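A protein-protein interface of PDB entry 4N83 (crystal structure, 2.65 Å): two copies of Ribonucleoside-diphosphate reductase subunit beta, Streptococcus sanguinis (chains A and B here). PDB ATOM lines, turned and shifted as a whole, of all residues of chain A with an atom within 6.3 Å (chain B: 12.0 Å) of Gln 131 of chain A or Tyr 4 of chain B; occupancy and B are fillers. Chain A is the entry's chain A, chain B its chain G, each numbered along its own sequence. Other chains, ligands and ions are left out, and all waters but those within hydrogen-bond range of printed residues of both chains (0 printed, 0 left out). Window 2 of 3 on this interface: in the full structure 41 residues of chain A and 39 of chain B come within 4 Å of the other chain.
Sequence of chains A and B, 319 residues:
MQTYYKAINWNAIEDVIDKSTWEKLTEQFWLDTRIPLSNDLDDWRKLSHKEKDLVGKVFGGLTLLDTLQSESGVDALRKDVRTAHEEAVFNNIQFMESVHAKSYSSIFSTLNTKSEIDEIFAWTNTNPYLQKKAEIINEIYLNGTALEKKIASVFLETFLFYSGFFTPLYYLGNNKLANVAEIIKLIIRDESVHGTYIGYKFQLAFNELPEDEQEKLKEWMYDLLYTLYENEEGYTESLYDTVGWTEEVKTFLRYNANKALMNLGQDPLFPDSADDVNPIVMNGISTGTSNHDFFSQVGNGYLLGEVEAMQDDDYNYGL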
ATOM      1  N   LEU A  64      18.731  16.605  22.639  1.00  0.00           N
ATOM      2  CA  LEU A  64      17.418  16.030  22.926  1.00  0.00           C
ATOM      3  C   LEU A  64      17.016  16.258  24.385  1.00  0.00           C
ATOM      4  O   LEU A  64      15.851  16.525  24.679  1.00  0.00           O
ATOM      5  CB  LEU A  64      17.422  14.527  22.621  1.00  0.00           C
ATOM      6  CG  LEU A  64      16.074  13.803  22.631  1.00  0.00           C
ATOM      7  CD1 LEU A  64      15.247  14.180  21.410  1.00  0.00           C
ATOM      8  CD2 LEU A  64      16.283  12.298  22.688  1.00  0.00           C
ATOM      9  N   THR A 124      19.204  11.054  16.126  1.00  0.00           N
ATOM     10  CA  THR A 124      18.925  11.308  17.543  1.00  0.00           C
ATOM     11  C   THR A 124      17.435  11.181  17.857  1.00  0.00           C
ATOM     12  O   THR A 124      17.060  10.784  18.962  1.00  0.00           O
ATOM     13  CB  THR A 124      19.404  12.706  17.985  1.00  0.00           C
ATOM     14  OG1 THR A 124      18.771  13.711  17.182  1.00  0.00           O
ATOM     15  CG2 THR A 124      20.914  12.831  17.852  1.00  0.00           C
ATOM     16  N   ASN A 125      16.595  11.521  16.880  1.00  0.00           N
ATOM     17  CA  ASN A 125      15.143  11.406  17.021  1.00  0.00           C
ATOM     18  C   ASN A 125      14.619   9.978  16.814  1.00  0.00           C
ATOM     19  O   ASN A 125      13.457   9.697  17.116  1.00  0.00           O
ATOM     20  CB  ASN A 125      14.438  12.362  16.051  1.00  0.00           C
ATOM     21  CG  ASN A 125      14.747  13.823  16.337  1.00  0.00           C
ATOM     22  OD1 ASN A 125      15.007  14.207  17.479  1.00  0.00           O
ATOM     23  ND2 ASN A 125      14.715  14.649  15.296  1.00  0.00           N
ATOM     24  N   THR A 126      15.470   9.088  16.300  1.00  0.00           N
ATOM     25  CA  THR A 126      15.103   7.686  16.071  1.00  0.00           C
ATOM     26  C   THR A 126      16.040   6.715  16.805  1.00  0.00           C
ATOM     27  O   THR A 126      16.188   5.560  16.403  1.00  0.00           O
ATOM     28  CB  THR A 126      15.114   7.351  14.565  1.00  0.00           C
ATOM     29  OG1 THR A 126      16.433   7.542  14.037  1.00  0.00           O
ATOM     30  CG2 THR A 126      14.131   8.236  13.807  1.00  0.00           C
ATOM     31  N   ASN A 127      16.659   7.188  17.883  1.00  0.00           N
ATOM     32  CA  ASN A 127      17.574   6.373  18.677  1.00  0.00           C
ATOM     33  C   ASN A 127      16.785   5.455  19.620  1.00  0.00           C
ATOM     34  O   ASN A 127      15.836   5.909  20.259  1.00  0.00           O
ATOM     35  CB  ASN A 127      18.507   7.286  19.479  1.00  0.00           C
ATOM     36  CG  ASN A 127      19.708   6.553  20.060  1.00  0.00           C
ATOM     37  OD1 ASN A 127      19.568   5.521  20.714  1.00  0.00           O
ATOM     38  ND2 ASN A 127      20.897   7.101  19.841  1.00  0.00           N
ATOM     39  N   PRO A 128      17.159   4.160  19.700  1.00  0.00           N
ATOM     40  CA  PRO A 128      16.529   3.259  20.678  1.00  0.00           C
ATOM     41  C   PRO A 128      16.791   3.630  22.143  1.00  0.00           C
ATOM     42  O   PRO A 128      15.902   3.478  22.982  1.00  0.00           O
ATOM     43  CB  PRO A 128      17.162   1.896  20.368  1.00  0.00           C
ATOM     44  CG  PRO A 128      17.647   1.998  18.967  1.00  0.00           C
ATOM     45  CD  PRO A 128      18.048   3.430  18.778  1.00  0.00           C
ATOM     46  N   TYR A 129      17.999   4.107  22.440  1.00  0.00           N
ATOM     47  CA  TYR A 129      18.399   4.417  23.815  1.00  0.00           C
ATOM     48  C   TYR A 129      17.862   5.768  24.281  1.00  0.00           C
ATOM     49  O   TYR A 129      17.214   5.853  25.323  1.00  0.00           O
ATOM     50  CB  TYR A 129      19.924   4.408  23.946  1.00  0.00           C
ATOM     51  CG  TYR A 129      20.571   3.105  23.535  1.00  0.00           C
ATOM     52  CD1 TYR A 129      20.549   1.998  24.380  1.00  0.00           C
ATOM     53  CD2 TYR A 129      21.210   2.979  22.304  1.00  0.00           C
ATOM     54  CE1 TYR A 129      21.142   0.802  24.009  1.00  0.00           C
ATOM     55  CE2 TYR A 129      21.806   1.788  21.924  1.00  0.00           C
ATOM     56  CZ  TYR A 129      21.769   0.704  22.779  1.00  0.00           C
ATOM     57  OH  TYR A 129      22.361  -0.481  22.406  1.00  0.00           O
ATOM     58  N   LEU A 130      18.135   6.813  23.502  1.00  0.00           N
ATOM     59  CA  LEU A 130      17.785   8.189  23.878  1.00  0.00           C
ATOM     60  C   LEU A 130      16.278   8.396  24.026  1.00  0.00           C
ATOM     61  O   LEU A 130      15.828   9.052  24.966  1.00  0.00           O
ATOM     62  CB  LEU A 130      18.333   9.187  22.851  1.00  0.00           C
ATOM     63  CG  LEU A 130      19.850   9.237  22.643  1.00  0.00           C
ATOM     64  CD1 LEU A 130      20.189  10.046  21.401  1.00  0.00           C
ATOM     65  CD2 LEU A 130      20.549   9.808  23.868  1.00  0.00           C
ATOM     66  N   GLN A 131      15.507   7.842  23.089  1.00  0.00           N
ATOM     67  CA  GLN A 131      14.045   7.948  23.120  1.00  0.00           C
ATOM     68  C   GLN A 131      13.450   7.242  24.336  1.00  0.00           C
ATOM     69  O   GLN A 131      12.506   7.744  24.946  1.00  0.00           O
ATOM     70  CB  GLN A 131      13.429   7.373  21.840  1.00  0.00           C
ATOM     71  CG  GLN A 131      13.709   8.192  20.588  1.00  0.00           C
ATOM     72  CD  GLN A 131      13.010   9.541  20.597  1.00  0.00           C
ATOM     73  OE1 GLN A 131      11.886   9.667  21.083  1.00  0.00           O
ATOM     74  NE2 GLN A 131      13.673  10.557  20.055  1.00  0.00           N
ATOM     75  N   LYS A 132      14.004   6.082  24.680  1.00  0.00           N
ATOM     76  CA  LYS A 132      13.571   5.342  25.866  1.00  0.00           C
ATOM     77  C   LYS A 132      14.072   6.049  27.128  1.00  0.00           C
ATOM     78  O   LYS A 132      13.360   6.121  28.130  1.00  0.00           O
ATOM     79  CB  LYS A 132      14.076   3.892  25.812  1.00  0.00           C
ATOM     80  CG  LYS A 132      13.180   2.878  26.514  1.00  0.00           C
ATOM     81  CD  LYS A 132      13.475   2.771  28.001  1.00  0.00           C
ATOM     82  CE  LYS A 132      12.586   1.736  28.673  1.00  0.00           C
ATOM     83  NZ  LYS A 132      11.167   2.179  28.770  1.00  0.00           N
ATOM     84  N   LYS A 133      15.293   6.578  27.062  1.00  0.00           N
ATOM     85  CA  LYS A 133      15.885   7.336  28.168  1.00  0.00           C
ATOM     86  C   LYS A 133      15.064   8.583  28.494  1.00  0.00           C
ATOM     87  O   LYS A 133      14.810   8.875  29.663  1.00  0.00           O
ATOM     88  CB  LYS A 133      17.328   7.726  27.826  1.00  0.00           C
ATOM     89  CG  LYS A 133      18.080   8.438  28.940  1.00  0.00           C
ATOM     90  CD  LYS A 133      19.587   8.405  28.714  1.00  0.00           C
ATOM     91  CE  LYS A 133      19.993   9.156  27.455  1.00  0.00           C
ATOM     92  NZ  LYS A 133      21.472   9.290  27.328  1.00  0.00           N
ATOM     93  N   ALA A 134      14.649   9.308  27.457  1.00  0.00           N
ATOM     94  CA  ALA A 134      13.801  10.491  27.622  1.00  0.00           C
ATOM     95  C   ALA A 134      12.381  10.126  28.068  1.00  0.00           C
ATOM     96  O   ALA A 134      11.733  10.899  28.777  1.00  0.00           O
ATOM     97  CB  ALA A 134      13.758  11.294  26.331  1.00  0.00           C
ATOM     98  N   GLU A 135      11.903   8.953  27.648  1.00  0.00           N
ATOM     99  CA  GLU A 135      10.561   8.478  28.005  1.00  0.00           C
ATOM    100  C   GLU A 135      10.441   8.193  29.502  1.00  0.00           C
ATOM    101  O   GLU A 135       9.415   8.497  30.111  1.00  0.00           O
ATOM    102  CB  GLU A 135      10.207   7.214  27.213  1.00  0.00           C
ATOM    103  CG  GLU A 135       8.739   6.811  27.294  1.00  0.00           C
ATOM    104  CD  GLU A 135       8.480   5.397  26.802  1.00  0.00           C
ATOM    105  OE1 GLU A 135       9.325   4.847  26.063  1.00  0.00           O
ATOM    106  OE2 GLU A 135       7.422   4.834  27.153  1.00  0.00           O
ATOM    107  N   ILE A 136      11.484   7.605  30.085  1.00  0.00           N
ATOM    108  CA  ILE A 136      11.512   7.321  31.521  1.00  0.00           C
ATOM    109  C   ILE A 136      11.490   8.620  32.329  1.00  0.00           C
ATOM    110  O   ILE A 136      10.816   8.706  33.355  1.00  0.00           O
ATOM    111  CB  ILE A 136      12.754   6.485  31.916  1.00  0.00           C
ATOM    112  CG1 ILE A 136      12.673   5.085  31.297  1.00  0.00           C
ATOM    113  CG2 ILE A 136      12.872   6.369  33.433  1.00  0.00           C
ATOM    114  CD1 ILE A 136      13.990   4.338  31.287  1.00  0.00           C
ATOM    115  N   ASN A 138      10.570  11.900  31.220  1.00  0.00           N
ATOM    116  CA  ASN A 138       9.391  12.745  30.987  1.00  0.00           C
ATOM    117  C   ASN A 138       8.126  12.179  31.632  1.00  0.00           C
ATOM    118  O   ASN A 138       7.261  12.934  32.079  1.00  0.00           O
ATOM    119  CB  ASN A 138       9.154  12.961  29.489  1.00  0.00           C
ATOM    120  CG  ASN A 138       8.159  14.079  29.204  1.00  0.00           C
ATOM    121  OD1 ASN A 138       7.959  14.979  30.021  1.00  0.00           O
ATOM    122  ND2 ASN A 138       7.534  14.028  28.034  1.00  0.00           N
ATOM    123  N   GLU A 139       8.024  10.850  31.672  1.00  0.00           N
ATOM    124  CA  GLU A 139       6.922  10.172  32.359  1.00  0.00           C
ATOM    125  C   GLU A 139       6.903  10.538  33.844  1.00  0.00           C
ATOM    126  O   GLU A 139       5.834  10.675  34.441  1.00  0.00           O
ATOM    127  CB  GLU A 139       7.033   8.650  32.177  1.00  0.00           C
ATOM    128  CG  GLU A 139       5.927   7.834  32.841  1.00  0.00           C
ATOM    129  CD  GLU A 139       6.208   7.495  34.297  1.00  0.00           C
ATOM    130  OE1 GLU A 139       7.377   7.209  34.644  1.00  0.00           O
ATOM    131  OE2 GLU A 139       5.251   7.506  35.101  1.00  0.00           O
ATOM    132  N   LEU A 142       5.626  14.197  34.015  1.00  0.00           N
ATOM    133  CA  LEU A 142       4.189  14.271  33.751  1.00  0.00           C
ATOM    134  C   LEU A 142       3.340  13.655  34.870  1.00  0.00           C
ATOM    135  O   LEU A 142       2.264  14.167  35.176  1.00  0.00           O
ATOM    136  CB  LEU A 142       3.852  13.608  32.406  1.00  0.00           C
ATOM    137  CG  LEU A 142       4.359  14.315  31.143  1.00  0.00           C
ATOM    138  CD1 LEU A 142       4.193  13.422  29.920  1.00  0.00           C
ATOM    139  CD2 LEU A 142       3.649  15.645  30.931  1.00  0.00           C
ATOM    140  N   TYR B   4       8.981   9.445  20.761  1.00  0.00           N
ATOM    141  CA  TYR B   4       8.248  10.005  21.939  1.00  0.00           C
ATOM    142  C   TYR B   4       8.470  11.511  22.096  1.00  0.00           C
ATOM    143  O   TYR B   4       7.519  12.256  22.339  1.00  0.00           O
ATOM    144  CB  TYR B   4       8.662   9.277  23.223  1.00  0.00           C
ATOM    145  CG  TYR B   4       7.886   9.710  24.449  1.00  0.00           C
ATOM    146  CD1 TYR B   4       8.476  10.511  25.424  1.00  0.00           C
ATOM    147  CD2 TYR B   4       6.558   9.324  24.630  1.00  0.00           C
ATOM    148  CE1 TYR B   4       7.769  10.911  26.544  1.00  0.00           C
ATOM    149  CE2 TYR B   4       5.843   9.720  25.749  1.00  0.00           C
ATOM    150  CZ  TYR B   4       6.451  10.513  26.703  1.00  0.00           C
ATOM    151  OH  TYR B   4       5.745  10.909  27.817  1.00  0.00           O
ATOM    152  N   TYR B   5       9.724  11.948  21.964  1.00  0.00           N
ATOM    153  CA  TYR B   5      10.079  13.365  22.073  1.00  0.00           C
ATOM    154  C   TYR B   5      10.974  13.783  20.906  1.00  0.00           C
ATOM    155  O   TYR B   5      11.722  12.966  20.371  1.00  0.00           O
ATOM    156  CB  TYR B   5      10.789  13.633  23.403  1.00  0.00           C
ATOM    157  CG  TYR B   5      10.379  14.929  24.062  1.00  0.00           C
ATOM    158  CD1 TYR B   5      11.021  16.126  23.758  1.00  0.00           C
ATOM    159  CD2 TYR B   5       9.342  14.957  24.991  1.00  0.00           C
ATOM    160  CE1 TYR B   5      10.641  17.314  24.363  1.00  0.00           C
ATOM    161  CE2 TYR B   5       8.955  16.138  25.601  1.00  0.00           C
ATOM    162  CZ  TYR B   5       9.606  17.314  25.284  1.00  0.00           C
ATOM    163  OH  TYR B   5       9.222  18.489  25.891  1.00  0.00           O
ATOM    164  N   LYS B   6      10.900  15.057  20.524  1.00  0.00           N
ATOM    165  CA  LYS B   6      11.676  15.579  19.399  1.00  0.00           C
ATOM    166  C   LYS B   6      12.657  16.656  19.851  1.00  0.00           C
ATOM    167  O   LYS B   6      12.351  17.457  20.733  1.00  0.00           O
ATOM    168  CB  LYS B   6      10.748  16.143  18.321  1.00  0.00           C
ATOM    169  CG  LYS B   6       9.666  15.171  17.868  1.00  0.00           C
ATOM    170  CD  LYS B   6       9.280  15.371  16.410  1.00  0.00           C
ATOM    171  CE  LYS B   6      10.303  14.751  15.469  1.00  0.00           C
ATOM    172  NZ  LYS B   6       9.838  14.745  14.054  1.00  0.00           N
ATOM    173  N   ALA B   7      13.836  16.667  19.232  1.00  0.00           N
ATOM    174  CA  ALA B   7      14.876  17.639  19.555  1.00  0.00           C
ATOM    175  C   ALA B   7      14.622  18.958  18.829  1.00  0.00           C
ATOM    176  O   ALA B   7      14.120  18.966  17.702  1.00  0.00           O
ATOM    177  CB  ALA B   7      16.246  17.089  19.185  1.00  0.00           C
ATOM    178  N   ILE B   8      14.971  20.065  19.482  1.00  0.00           N
ATOM    179  CA  ILE B   8      14.814  21.397  18.896  1.00  0.00           C
ATOM    180  C   ILE B   8      15.984  21.694  17.956  1.00  0.00           C
ATOM    181  O   ILE B   8      17.142  21.422  18.287  1.00  0.00           O
ATOM    182  CB  ILE B   8      14.687  22.492  19.984  1.00  0.00           C
ATOM    183  CG1 ILE B   8      14.166  23.796  19.374  1.00  0.00           C
ATOM    184  CG2 ILE B   8      16.011  22.729  20.704  1.00  0.00           C
ATOM    185  CD1 ILE B   8      13.764  24.830  20.404  1.00  0.00           C
ATOM    186  N   ALA B  84       8.607  24.799  17.889  1.00  0.00           N
ATOM    187  CA  ALA B  84       9.432  24.439  19.046  1.00  0.00           C
ATOM    188  C   ALA B  84      10.326  25.603  19.494  1.00  0.00           C
ATOM    189  O   ALA B  84      10.714  25.682  20.662  1.00  0.00           O
ATOM    190  CB  ALA B  84      10.278  23.214  18.729  1.00  0.00           C
ATOM    191  N   GLU B  87       8.463  28.259  21.972  1.00  0.00           N
ATOM    192  CA  GLU B  87       8.452  27.921  23.397  1.00  0.00           C
ATOM    193  C   GLU B  87       9.757  28.348  24.065  1.00  0.00           C
ATOM    194  O   GLU B  87       9.758  28.734  25.234  1.00  0.00           O
ATOM    195  CB  GLU B  87       8.209  26.423  23.617  1.00  0.00           C
ATOM    196  CG  GLU B  87       7.916  26.066  25.073  1.00  0.00           C
ATOM    197  CD  GLU B  87       7.562  24.601  25.284  1.00  0.00           C
ATOM    198  OE1 GLU B  87       7.572  23.826  24.306  1.00  0.00           O
ATOM    199  OE2 GLU B  87       7.273  24.226  26.441  1.00  0.00           O
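Of chain B, only Tyr 4 (2.9 Å) and Tyr 5 (3.1 Å) come within 4 Å of Gln 131 of chain A. Tyr 4 of chain B touches just these residues of chain A: Gln 131 (2.9 Å), Glu 135 (3.9 Å), Asn 138 (3.5 Å) and Leu 142 (3.6 Å). Of the printed residues of chain B, Asn 125 of chain A touches Ala 7. No residue of chain B comes within 4 Å of Asn 127 of chain A. No residue of chain B comes within 4 Å of Leu 130 of chain A. Lys 133 of chain A touches none of the printed residues of chain B. No residue of chain B comes within 4 Å of Ala 134 of chain A. Of the printed residues of chain B, Glu 135 of chain A touches Tyr 4 (3.9 Å). Asn 138 of chain A touches just these residues of chain B: Tyr 4 and Tyr 5. Printed residues of chain A within 4 Å of Tyr 5 of chain B: Leu 64, Gln 131 and Asn 138. Of the printed residues of chain A, Ala 7 of chain B touches Leu 64 (3.6 Å) and Asn 125 (3.2 Å). Glu 139 of chain A touches none of the printed residues of chain B. The nearest residue of chain B that does not touch Gln 131 of chain A is Lys 6 of chain B (5.3 Å). The nearest residue of chain A that does not touch Tyr 4 of chain B is Glu 139 of chain A (4.5 Å). The nearest printed residue of chain B that does not touch Leu 142 of chain A is Tyr 5 of chain B (7.0 Å).
NE2 of Gln 131 of chain A sits at hydrogen-bond distance from O of Tyr 5 of chain B. The side-chain amide oxygen of Gln 131 of chain A lies within hydrogen-bond range of the backbone NH of Tyr 4 of chain B, 2.9 Å away. OD1 of Asn 125 of chain A sits at hydrogen-bond distance from N of Ala 7 of chain B (3.2 Å).
The side-chain amide nitrogen of Gln 131 of chain A is in hydrogen-bond range of the backbone carbonyl oxygen of Asn 125 of chain A (3.1 Å).
Among the printed residues, pairs that only touch across the chains: Asn 138 of chain A with Tyr 4 of chain B, Asn 138 of chain A with Tyr 5 of chain B, Leu 64 of chain A with Ala 7 of chain B, Leu 142 of chain A with Tyr 4 of chain B, Leu 64 of chain A with Tyr 5 of chain B, Glu 135 of chain A with Tyr 4 of chain B and Leu 64 of chain A with Lys 6 of chain B.
Hydrophobic or aromatic side chains of chain B within 4 Å of the printed part of chain A: Tyr 4, Tyr 5 and Ala 7. Of the 17 printed residues of chain A, 6 touch a printed residue of chain B. Hydrophobic or aromatic side chains of chain A within 4 Å of the printed part of chain B: Leu 64 and Leu 142. Among the printed residues, 10 pairs touch across the chains. Among the printed residues, no Asp or Glu carboxylate lies within 4 Å of a Lys or Arg side-chain nitrogen of the other chain.
No position is printed for both chains.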
